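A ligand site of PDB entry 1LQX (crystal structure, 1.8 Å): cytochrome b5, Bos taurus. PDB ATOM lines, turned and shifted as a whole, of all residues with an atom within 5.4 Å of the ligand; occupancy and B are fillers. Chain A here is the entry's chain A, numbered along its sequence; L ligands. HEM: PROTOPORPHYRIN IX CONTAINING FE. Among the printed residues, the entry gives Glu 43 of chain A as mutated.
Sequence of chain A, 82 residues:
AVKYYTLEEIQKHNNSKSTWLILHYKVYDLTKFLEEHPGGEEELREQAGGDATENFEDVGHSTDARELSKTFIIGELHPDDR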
ATOM      1  N   LEU A  21       7.786 -15.513 -22.822  1.00  0.00           N
ATOM      2  CA  LEU A  21       6.972 -16.289 -21.910  1.00  0.00           C
ATOM      3  C   LEU A  21       7.877 -16.815 -20.802  1.00  0.00           C
ATOM      4  O   LEU A  21       9.097 -16.823 -20.937  1.00  0.00           O
ATOM      5  CB  LEU A  21       6.214 -17.413 -22.629  1.00  0.00           C
ATOM      6  CG  LEU A  21       6.903 -18.481 -23.457  1.00  0.00           C
ATOM      7  CD1 LEU A  21       7.644 -19.455 -22.556  1.00  0.00           C
ATOM      8  CD2 LEU A  21       5.843 -19.214 -24.267  1.00  0.00           C
ATOM      9  N   LEU A  23       8.984 -19.883 -18.099  1.00  0.00           N
ATOM     10  CA  LEU A  23       9.000 -21.316 -17.837  1.00  0.00           C
ATOM     11  C   LEU A  23       9.932 -21.539 -16.648  1.00  0.00           C
ATOM     12  O   LEU A  23      11.131 -21.248 -16.744  1.00  0.00           O
ATOM     13  CB  LEU A  23       9.537 -22.111 -19.037  1.00  0.00           C
ATOM     14  CG  LEU A  23       8.755 -22.095 -20.345  1.00  0.00           C
ATOM     15  CD1 LEU A  23       9.520 -22.921 -21.387  1.00  0.00           C
ATOM     16  CD2 LEU A  23       7.355 -22.650 -20.155  1.00  0.00           C
ATOM     17  N   TYR A  28      11.934 -16.519 -21.553  1.00  0.00           N
ATOM     18  CA  TYR A  28      12.383 -16.941 -22.875  1.00  0.00           C
ATOM     19  C   TYR A  28      11.848 -16.013 -23.951  1.00  0.00           C
ATOM     20  O   TYR A  28      10.691 -15.617 -23.908  1.00  0.00           O
ATOM     21  CB  TYR A  28      11.882 -18.359 -23.187  1.00  0.00           C
ATOM     22  CG  TYR A  28      12.369 -19.423 -22.243  1.00  0.00           C
ATOM     23  CD1 TYR A  28      11.886 -19.505 -20.938  1.00  0.00           C
ATOM     24  CD2 TYR A  28      13.327 -20.345 -22.650  1.00  0.00           C
ATOM     25  CE1 TYR A  28      12.355 -20.475 -20.054  1.00  0.00           C
ATOM     26  CE2 TYR A  28      13.810 -21.323 -21.773  1.00  0.00           C
ATOM     27  CZ  TYR A  28      13.313 -21.380 -20.488  1.00  0.00           C
ATOM     28  OH  TYR A  28      13.798 -22.335 -19.616  1.00  0.00           O
ATOM     29  N   LEU A  30      10.889 -16.184 -27.503  1.00  0.00           N
ATOM     30  CA  LEU A  30      10.617 -17.159 -28.558  1.00  0.00           C
ATOM     31  C   LEU A  30      10.183 -16.556 -29.882  1.00  0.00           C
ATOM     32  O   LEU A  30       9.686 -17.260 -30.763  1.00  0.00           O
ATOM     33  CB  LEU A  30       9.533 -18.138 -28.093  1.00  0.00           C
ATOM     34  CG  LEU A  30       9.812 -18.882 -26.791  1.00  0.00           C
ATOM     35  CD1 LEU A  30       8.638 -19.810 -26.480  1.00  0.00           C
ATOM     36  CD2 LEU A  30      11.109 -19.662 -26.905  1.00  0.00           C
ATOM     37  N   PHE A  33      11.443 -18.388 -32.806  1.00  0.00           N
ATOM     38  CA  PHE A  33      11.196 -19.819 -32.723  1.00  0.00           C
ATOM     39  C   PHE A  33       9.773 -20.208 -33.106  1.00  0.00           C
ATOM     40  O   PHE A  33       9.493 -21.359 -33.426  1.00  0.00           O
ATOM     41  CB  PHE A  33      11.515 -20.302 -31.290  1.00  0.00           C
ATOM     42  CG  PHE A  33      11.301 -21.773 -31.073  1.00  0.00           C
ATOM     43  CD1 PHE A  33      10.328 -22.217 -30.178  1.00  0.00           C
ATOM     44  CD2 PHE A  33      12.071 -22.708 -31.744  1.00  0.00           C
ATOM     45  CE1 PHE A  33      10.129 -23.572 -29.968  1.00  0.00           C
ATOM     46  CE2 PHE A  33      11.883 -24.073 -31.532  1.00  0.00           C
ATOM     47  CZ  PHE A  33      10.899 -24.507 -30.639  1.00  0.00           C
ATOM     48  N   HIS A  37       8.739 -24.171 -34.113  1.00  0.00           N
ATOM     49  CA  HIS A  37       8.181 -25.012 -33.063  1.00  0.00           C
ATOM     50  C   HIS A  37       7.329 -26.167 -33.595  1.00  0.00           C
ATOM     51  O   HIS A  37       6.287 -25.943 -34.218  1.00  0.00           O
ATOM     52  CB  HIS A  37       7.338 -24.158 -32.121  1.00  0.00           C
ATOM     53  CG  HIS A  37       6.755 -24.921 -30.972  1.00  0.00           C
ATOM     54  ND1 HIS A  37       5.427 -24.872 -30.613  1.00  0.00           N
ATOM     55  CD2 HIS A  37       7.351 -25.750 -30.077  1.00  0.00           C
ATOM     56  CE1 HIS A  37       5.258 -25.648 -29.538  1.00  0.00           C
ATOM     57  NE2 HIS A  37       6.396 -26.194 -29.175  1.00  0.00           N
ATOM     58  N   PRO A  38       7.746 -27.428 -33.363  1.00  0.00           N
ATOM     59  CA  PRO A  38       6.999 -28.589 -33.835  1.00  0.00           C
ATOM     60  C   PRO A  38       5.534 -28.599 -33.402  1.00  0.00           C
ATOM     61  O   PRO A  38       4.667 -29.103 -34.119  1.00  0.00           O
ATOM     62  CB  PRO A  38       7.780 -29.765 -33.239  1.00  0.00           C
ATOM     63  CG  PRO A  38       9.183 -29.249 -33.217  1.00  0.00           C
ATOM     64  CD  PRO A  38       8.995 -27.841 -32.700  1.00  0.00           C
ATOM     65  N   GLY A  39       5.265 -28.033 -32.236  1.00  0.00           N
ATOM     66  CA  GLY A  39       3.902 -28.001 -31.730  1.00  0.00           C
ATOM     67  C   GLY A  39       3.044 -26.866 -32.268  1.00  0.00           C
ATOM     68  O   GLY A  39       1.923 -26.663 -31.798  1.00  0.00           O
ATOM     69  N   GLU A  43       0.102 -22.379 -29.992  1.00  0.00           N
ATOM     70  CA  GLU A  43       0.280 -22.800 -28.608  1.00  0.00           C
ATOM     71  C   GLU A  43       1.155 -21.797 -27.864  1.00  0.00           C
ATOM     72  O   GLU A  43       0.942 -21.518 -26.688  1.00  0.00           O
ATOM     73  CB  GLU A  43       0.942 -24.177 -28.544  1.00  0.00           C
ATOM     74  CG  GLU A  43       0.080 -25.322 -29.079  1.00  0.00           C
ATOM     75  CD  GLU A  43      -1.018 -25.730 -28.112  1.00  0.00           C
ATOM     76  OE1 GLU A  43      -1.817 -26.625 -28.465  1.00  0.00           O
ATOM     77  OE2 GLU A  43      -1.075 -25.167 -26.997  1.00  0.00           O
ATOM     78  N   LEU A  44       2.134 -21.242 -28.572  1.00  0.00           N
ATOM     79  CA  LEU A  44       3.058 -20.271 -27.984  1.00  0.00           C
ATOM     80  C   LEU A  44       2.437 -18.881 -27.873  1.00  0.00           C
ATOM     81  O   LEU A  44       2.559 -18.224 -26.830  1.00  0.00           O
ATOM     82  CB  LEU A  44       4.341 -20.212 -28.807  1.00  0.00           C
ATOM     83  CG  LEU A  44       5.064 -21.545 -29.039  1.00  0.00           C
ATOM     84  CD1 LEU A  44       6.394 -21.298 -29.726  1.00  0.00           C
ATOM     85  CD2 LEU A  44       5.282 -22.237 -27.713  1.00  0.00           C
ATOM     86  N   GLN A  47       0.074 -18.228 -24.945  1.00  0.00           N
ATOM     87  CA  GLN A  47       0.704 -18.123 -23.630  1.00  0.00           C
ATOM     88  C   GLN A  47       1.660 -16.945 -23.504  1.00  0.00           C
ATOM     89  O   GLN A  47       2.164 -16.653 -22.410  1.00  0.00           O
ATOM     90  CB  GLN A  47       1.473 -19.408 -23.312  1.00  0.00           C
ATOM     91  CG  GLN A  47       0.626 -20.671 -23.307  1.00  0.00           C
ATOM     92  CD  GLN A  47      -0.482 -20.624 -22.266  1.00  0.00           C
ATOM     93  OE1 GLN A  47      -0.224 -20.380 -21.092  1.00  0.00           O
ATOM     94  NE2 GLN A  47      -1.712 -20.862 -22.699  1.00  0.00           N
ATOM     95  N   ALA A  52       3.917 -20.119 -18.699  1.00  0.00           N
ATOM     96  CA  ALA A  52       3.383 -21.276 -19.419  1.00  0.00           C
ATOM     97  C   ALA A  52       3.989 -22.571 -18.900  1.00  0.00           C
ATOM     98  O   ALA A  52       3.966 -23.590 -19.604  1.00  0.00           O
ATOM     99  CB  ALA A  52       3.669 -21.125 -20.904  1.00  0.00           C
ATOM    100  N   ASN A  55       1.545 -25.700 -18.804  1.00  0.00           N
ATOM    101  CA  ASN A  55       1.224 -26.153 -20.158  1.00  0.00           C
ATOM    102  C   ASN A  55       2.399 -26.861 -20.787  1.00  0.00           C
ATOM    103  O   ASN A  55       2.242 -27.846 -21.501  1.00  0.00           O
ATOM    104  CB  ASN A  55       0.829 -24.964 -21.032  1.00  0.00           C
ATOM    105  CG  ASN A  55      -0.310 -24.157 -20.462  1.00  0.00           C
ATOM    106  OD1 ASN A  55      -0.126 -23.389 -19.519  1.00  0.00           O
ATOM    107  ND2 ASN A  55      -1.493 -24.342 -21.017  1.00  0.00           N
ATOM    108  N   PHE A  56       3.595 -26.325 -20.531  1.00  0.00           N
ATOM    109  CA  PHE A  56       4.831 -26.876 -21.061  1.00  0.00           C
ATOM    110  C   PHE A  56       5.071 -28.287 -20.517  1.00  0.00           C
ATOM    111  O   PHE A  56       5.468 -29.195 -21.249  1.00  0.00           O
ATOM    112  CB  PHE A  56       5.996 -25.970 -20.683  1.00  0.00           C
ATOM    113  CG  PHE A  56       7.333 -26.435 -21.194  1.00  0.00           C
ATOM    114  CD1 PHE A  56       7.687 -26.245 -22.521  1.00  0.00           C
ATOM    115  CD2 PHE A  56       8.236 -27.056 -20.335  1.00  0.00           C
ATOM    116  CE1 PHE A  56       8.924 -26.665 -22.993  1.00  0.00           C
ATOM    117  CE2 PHE A  56       9.478 -27.479 -20.794  1.00  0.00           C
ATOM    118  CZ  PHE A  56       9.826 -27.277 -22.132  1.00  0.00           C
ATOM    119  N   VAL A  59       2.328 -31.173 -21.579  1.00  0.00           N
ATOM    120  CA  VAL A  59       2.543 -31.839 -22.859  1.00  0.00           C
ATOM    121  C   VAL A  59       3.717 -32.811 -22.773  1.00  0.00           C
ATOM    122  O   VAL A  59       3.830 -33.734 -23.576  1.00  0.00           O
ATOM    123  CB  VAL A  59       2.798 -30.819 -23.978  1.00  0.00           C
ATOM    124  CG1 VAL A  59       1.573 -29.936 -24.185  1.00  0.00           C
ATOM    125  CG2 VAL A  59       3.980 -29.959 -23.618  1.00  0.00           C
ATOM    126  N   GLY A  60       4.585 -32.598 -21.791  1.00  0.00           N
ATOM    127  CA  GLY A  60       5.736 -33.465 -21.587  1.00  0.00           C
ATOM    128  C   GLY A  60       6.854 -33.411 -22.620  1.00  0.00           C
ATOM    129  O   GLY A  60       7.104 -34.402 -23.309  1.00  0.00           O
ATOM    130  N   HIS A  61       7.528 -32.264 -22.711  1.00  0.00           N
ATOM    131  CA  HIS A  61       8.615 -32.098 -23.660  1.00  0.00           C
ATOM    132  C   HIS A  61       9.793 -33.024 -23.417  1.00  0.00           C
ATOM    133  O   HIS A  61      10.112 -33.343 -22.283  1.00  0.00           O
ATOM    134  CB  HIS A  61       9.106 -30.649 -23.653  1.00  0.00           C
ATOM    135  CG  HIS A  61       8.191 -29.706 -24.353  1.00  0.00           C
ATOM    136  ND1 HIS A  61       7.015 -29.214 -23.816  1.00  0.00           N
ATOM    137  CD2 HIS A  61       8.253 -29.195 -25.608  1.00  0.00           C
ATOM    138  CE1 HIS A  61       6.432 -28.458 -24.747  1.00  0.00           C
ATOM    139  NE2 HIS A  61       7.135 -28.419 -25.846  1.00  0.00           N
ATOM    140  N   SER A  62      10.450 -33.426 -24.497  1.00  0.00           N
ATOM    141  CA  SER A  62      11.589 -34.325 -24.428  1.00  0.00           C
ATOM    142  C   SER A  62      12.835 -33.621 -23.908  1.00  0.00           C
ATOM    143  O   SER A  62      12.854 -32.395 -23.769  1.00  0.00           O
ATOM    144  CB  SER A  62      11.900 -34.897 -25.812  1.00  0.00           C
ATOM    145  OG  SER A  62      12.337 -33.872 -26.682  1.00  0.00           O
ATOM    146  N   ALA A  65      14.186 -31.166 -26.449  1.00  0.00           N
ATOM    147  CA  ALA A  65      13.437 -29.909 -26.513  1.00  0.00           C
ATOM    148  C   ALA A  65      13.877 -29.005 -25.367  1.00  0.00           C
ATOM    149  O   ALA A  65      14.020 -27.795 -25.550  1.00  0.00           O
ATOM    150  CB  ALA A  65      11.952 -30.189 -26.426  1.00  0.00           C
ATOM    151  N   LEU A  68      17.321 -27.486 -26.038  1.00  0.00           N
ATOM    152  CA  LEU A  68      17.218 -26.431 -27.034  1.00  0.00           C
ATOM    153  C   LEU A  68      16.612 -25.138 -26.468  1.00  0.00           C
ATOM    154  O   LEU A  68      17.026 -24.040 -26.829  1.00  0.00           O
ATOM    155  CB  LEU A  68      16.359 -26.905 -28.216  1.00  0.00           C
ATOM    156  CG  LEU A  68      15.986 -25.833 -29.234  1.00  0.00           C
ATOM    157  CD1 LEU A  68      17.242 -25.261 -29.885  1.00  0.00           C
ATOM    158  CD2 LEU A  68      15.047 -26.431 -30.270  1.00  0.00           C
ATOM    159  N   SER A  69      15.641 -25.284 -25.569  1.00  0.00           N
ATOM    160  CA  SER A  69      14.983 -24.124 -24.982  1.00  0.00           C
ATOM    161  C   SER A  69      15.980 -23.179 -24.305  1.00  0.00           C
ATOM    162  O   SER A  69      15.778 -21.971 -24.290  1.00  0.00           O
ATOM    163  CB  SER A  69      13.938 -24.563 -23.958  1.00  0.00           C
ATOM    164  OG  SER A  69      14.543 -25.040 -22.766  1.00  0.00           O
ATOM    165  N   PHE A  72      17.176 -19.823 -25.745  1.00  0.00           N
ATOM    166  CA  PHE A  72      16.279 -18.679 -25.819  1.00  0.00           C
ATOM    167  C   PHE A  72      16.119 -17.911 -24.513  1.00  0.00           C
ATOM    168  O   PHE A  72      15.383 -16.919 -24.455  1.00  0.00           O
ATOM    169  CB  PHE A  72      14.895 -19.143 -26.307  1.00  0.00           C
ATOM    170  CG  PHE A  72      14.941 -19.829 -27.647  1.00  0.00           C
ATOM    171  CD1 PHE A  72      15.310 -19.133 -28.798  1.00  0.00           C
ATOM    172  CD2 PHE A  72      14.621 -21.187 -27.762  1.00  0.00           C
ATOM    173  CE1 PHE A  72      15.379 -19.791 -30.033  1.00  0.00           C
ATOM    174  CE2 PHE A  72      14.686 -21.838 -28.985  1.00  0.00           C
ATOM    175  CZ  PHE A  72      15.065 -21.142 -30.133  1.00  0.00           C
HETATM  176  CHA HEM L   1       6.228 -30.221 -29.208  1.00  0.00           C
HETATM  177  CHB HEM L   1      10.158 -27.504 -28.393  1.00  0.00           C
HETATM  178  CHC HEM L   1       7.463 -24.563 -25.652  1.00  0.00           C
HETATM  179  CHD HEM L   1       3.465 -27.078 -26.727  1.00  0.00           C
HETATM  180  C1A HEM L   1       7.543 -29.782 -29.153  1.00  0.00           C
HETATM  181  C2A HEM L   1       8.670 -30.489 -29.712  1.00  0.00           C
HETATM  182  C3A HEM L   1       9.758 -29.697 -29.528  1.00  0.00           C
HETATM  183  C4A HEM L   1       9.304 -28.507 -28.831  1.00  0.00           C
HETATM  184  CMA HEM L   1      11.200 -29.978 -29.915  1.00  0.00           C
HETATM  185  CAA HEM L   1       8.705 -31.878 -30.360  1.00  0.00           C
HETATM  186  CBA HEM L   1       8.460 -33.019 -29.380  1.00  0.00           C
HETATM  187  CGA HEM L   1       9.401 -32.980 -28.206  1.00  0.00           C
HETATM  188  O1A HEM L   1      10.631 -32.968 -28.420  1.00  0.00           O
HETATM  189  O2A HEM L   1       8.923 -32.974 -27.051  1.00  0.00           O
HETATM  190  C1B HEM L   1       9.747 -26.466 -27.565  1.00  0.00           C
HETATM  191  C2B HEM L   1      10.641 -25.462 -27.035  1.00  0.00           C
HETATM  192  C3B HEM L   1       9.877 -24.625 -26.299  1.00  0.00           C
HETATM  193  C4B HEM L   1       8.537 -25.146 -26.320  1.00  0.00           C
HETATM  194  CMB HEM L   1      12.147 -25.342 -27.267  1.00  0.00           C
HETATM  195  CAB HEM L   1      10.301 -23.404 -25.794  1.00  0.00           C
HETATM  196  CBB HEM L   1      10.780 -23.233 -24.499  1.00  0.00           C
HETATM  197  C1C HEM L   1       6.149 -25.029 -25.682  1.00  0.00           C
HETATM  198  C2C HEM L   1       5.087 -24.430 -24.905  1.00  0.00           C
HETATM  199  C3C HEM L   1       3.935 -25.102 -25.225  1.00  0.00           C
HETATM  200  C4C HEM L   1       4.324 -26.130 -26.192  1.00  0.00           C
HETATM  201  CMC HEM L   1       5.224 -23.249 -23.936  1.00  0.00           C
HETATM  202  CAC HEM L   1       2.645 -24.906 -24.735  1.00  0.00           C
HETATM  203  CBC HEM L   1       2.133 -23.832 -24.003  1.00  0.00           C
HETATM  204  C1D HEM L   1       3.885 -28.134 -27.523  1.00  0.00           C
HETATM  205  C2D HEM L   1       3.002 -29.113 -28.109  1.00  0.00           C
HETATM  206  C3D HEM L   1       3.763 -29.997 -28.781  1.00  0.00           C
HETATM  207  C4D HEM L   1       5.136 -29.567 -28.628  1.00  0.00           C
HETATM  208  CMD HEM L   1       1.485 -29.123 -28.039  1.00  0.00           C
HETATM  209  CAD HEM L   1       3.235 -31.206 -29.545  1.00  0.00           C
HETATM  210  CBD HEM L   1       3.361 -32.488 -28.757  1.00  0.00           C
HETATM  211  CGD HEM L   1       2.630 -33.646 -29.409  1.00  0.00           C
HETATM  212  O1D HEM L   1       2.899 -33.940 -30.590  1.00  0.00           O
HETATM  213  O2D HEM L   1       1.782 -34.275 -28.736  1.00  0.00           O
HETATM  214  NA  HEM L   1       7.944 -28.573 -28.560  1.00  0.00           N
HETATM  215  NB  HEM L   1       8.451 -26.282 -27.114  1.00  0.00           N
HETATM  216  NC  HEM L   1       5.698 -26.097 -26.444  1.00  0.00           N
HETATM  217  ND  HEM L   1       5.210 -28.389 -27.883  1.00  0.00           N
HETATM  218 FE   HEM L   1       6.823 -27.330 -27.522  1.00  0.00          FE
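An iron atom (FE) of the ligand is bound by a ring nitrogen (NE2) of His 61 (2.0 Å). A ring nitrogen (NE2) of His 37 binds an iron atom (FE) of the ligand. The side-chain hydroxyl of Ser 62 sits at hydrogen-bond distance from an oxygen (O1A) of the ligand. The backbone NH of Ser 62 lies within hydrogen-bond range of an oxygen (O2A) of the ligand (3.0 Å).
The backbone NH (N) of Ala 65 lies within hydrogen-bond range of the side-chain hydroxyl (OG) of Ser 62. The side-chain amide oxygen of Gln 47 sits close to the side-chain amide oxygen of Asn 55. O of Phe 56 is in hydrogen-bond range of ND1 of His 61 (3.0 Å).
CD1 of Leu 23 touches CBB of the ligand, at 3.4 Å. CD2 of Leu 30 touches CAB of the ligand, 3.99 Å away. CE1 of Phe 33 touches C2B of the ligand, 3.5 Å away. Pro 38 touches the ligand (CB to CAA, 3.7 Å). CA of Gly 39 touches C3D of the ligand, 3.6 Å away. O of Glu 43 touches CBC of the ligand, 3.7 Å away. CD2 of Leu 44 touches C1C of the ligand (3.6 Å). Gln 47 touches the ligand (CG to CBC, 3.6 Å). Asn 55 touches the ligand (CB to CBC, 3.4 Å). Phe 56 touches the ligand. Val 59 touches the ligand (CG1 to CMD, 3.9 Å). Ala 65 touches the ligand (O to CMB, 3.5 Å). Ser 69 touches the ligand. Hydrophobic or aromatic side chains that line the ligand: Leu 23, Leu 30, Phe 33, His 37, Pro 38, Leu 44, Phe 56, Val 59, His 61 and Ala 65. Of the 22 residues printed, 16 come within 4 Å of the ligand. The nearest printed residue that does not touch the ligand is Ala 52 (4.02 Å).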
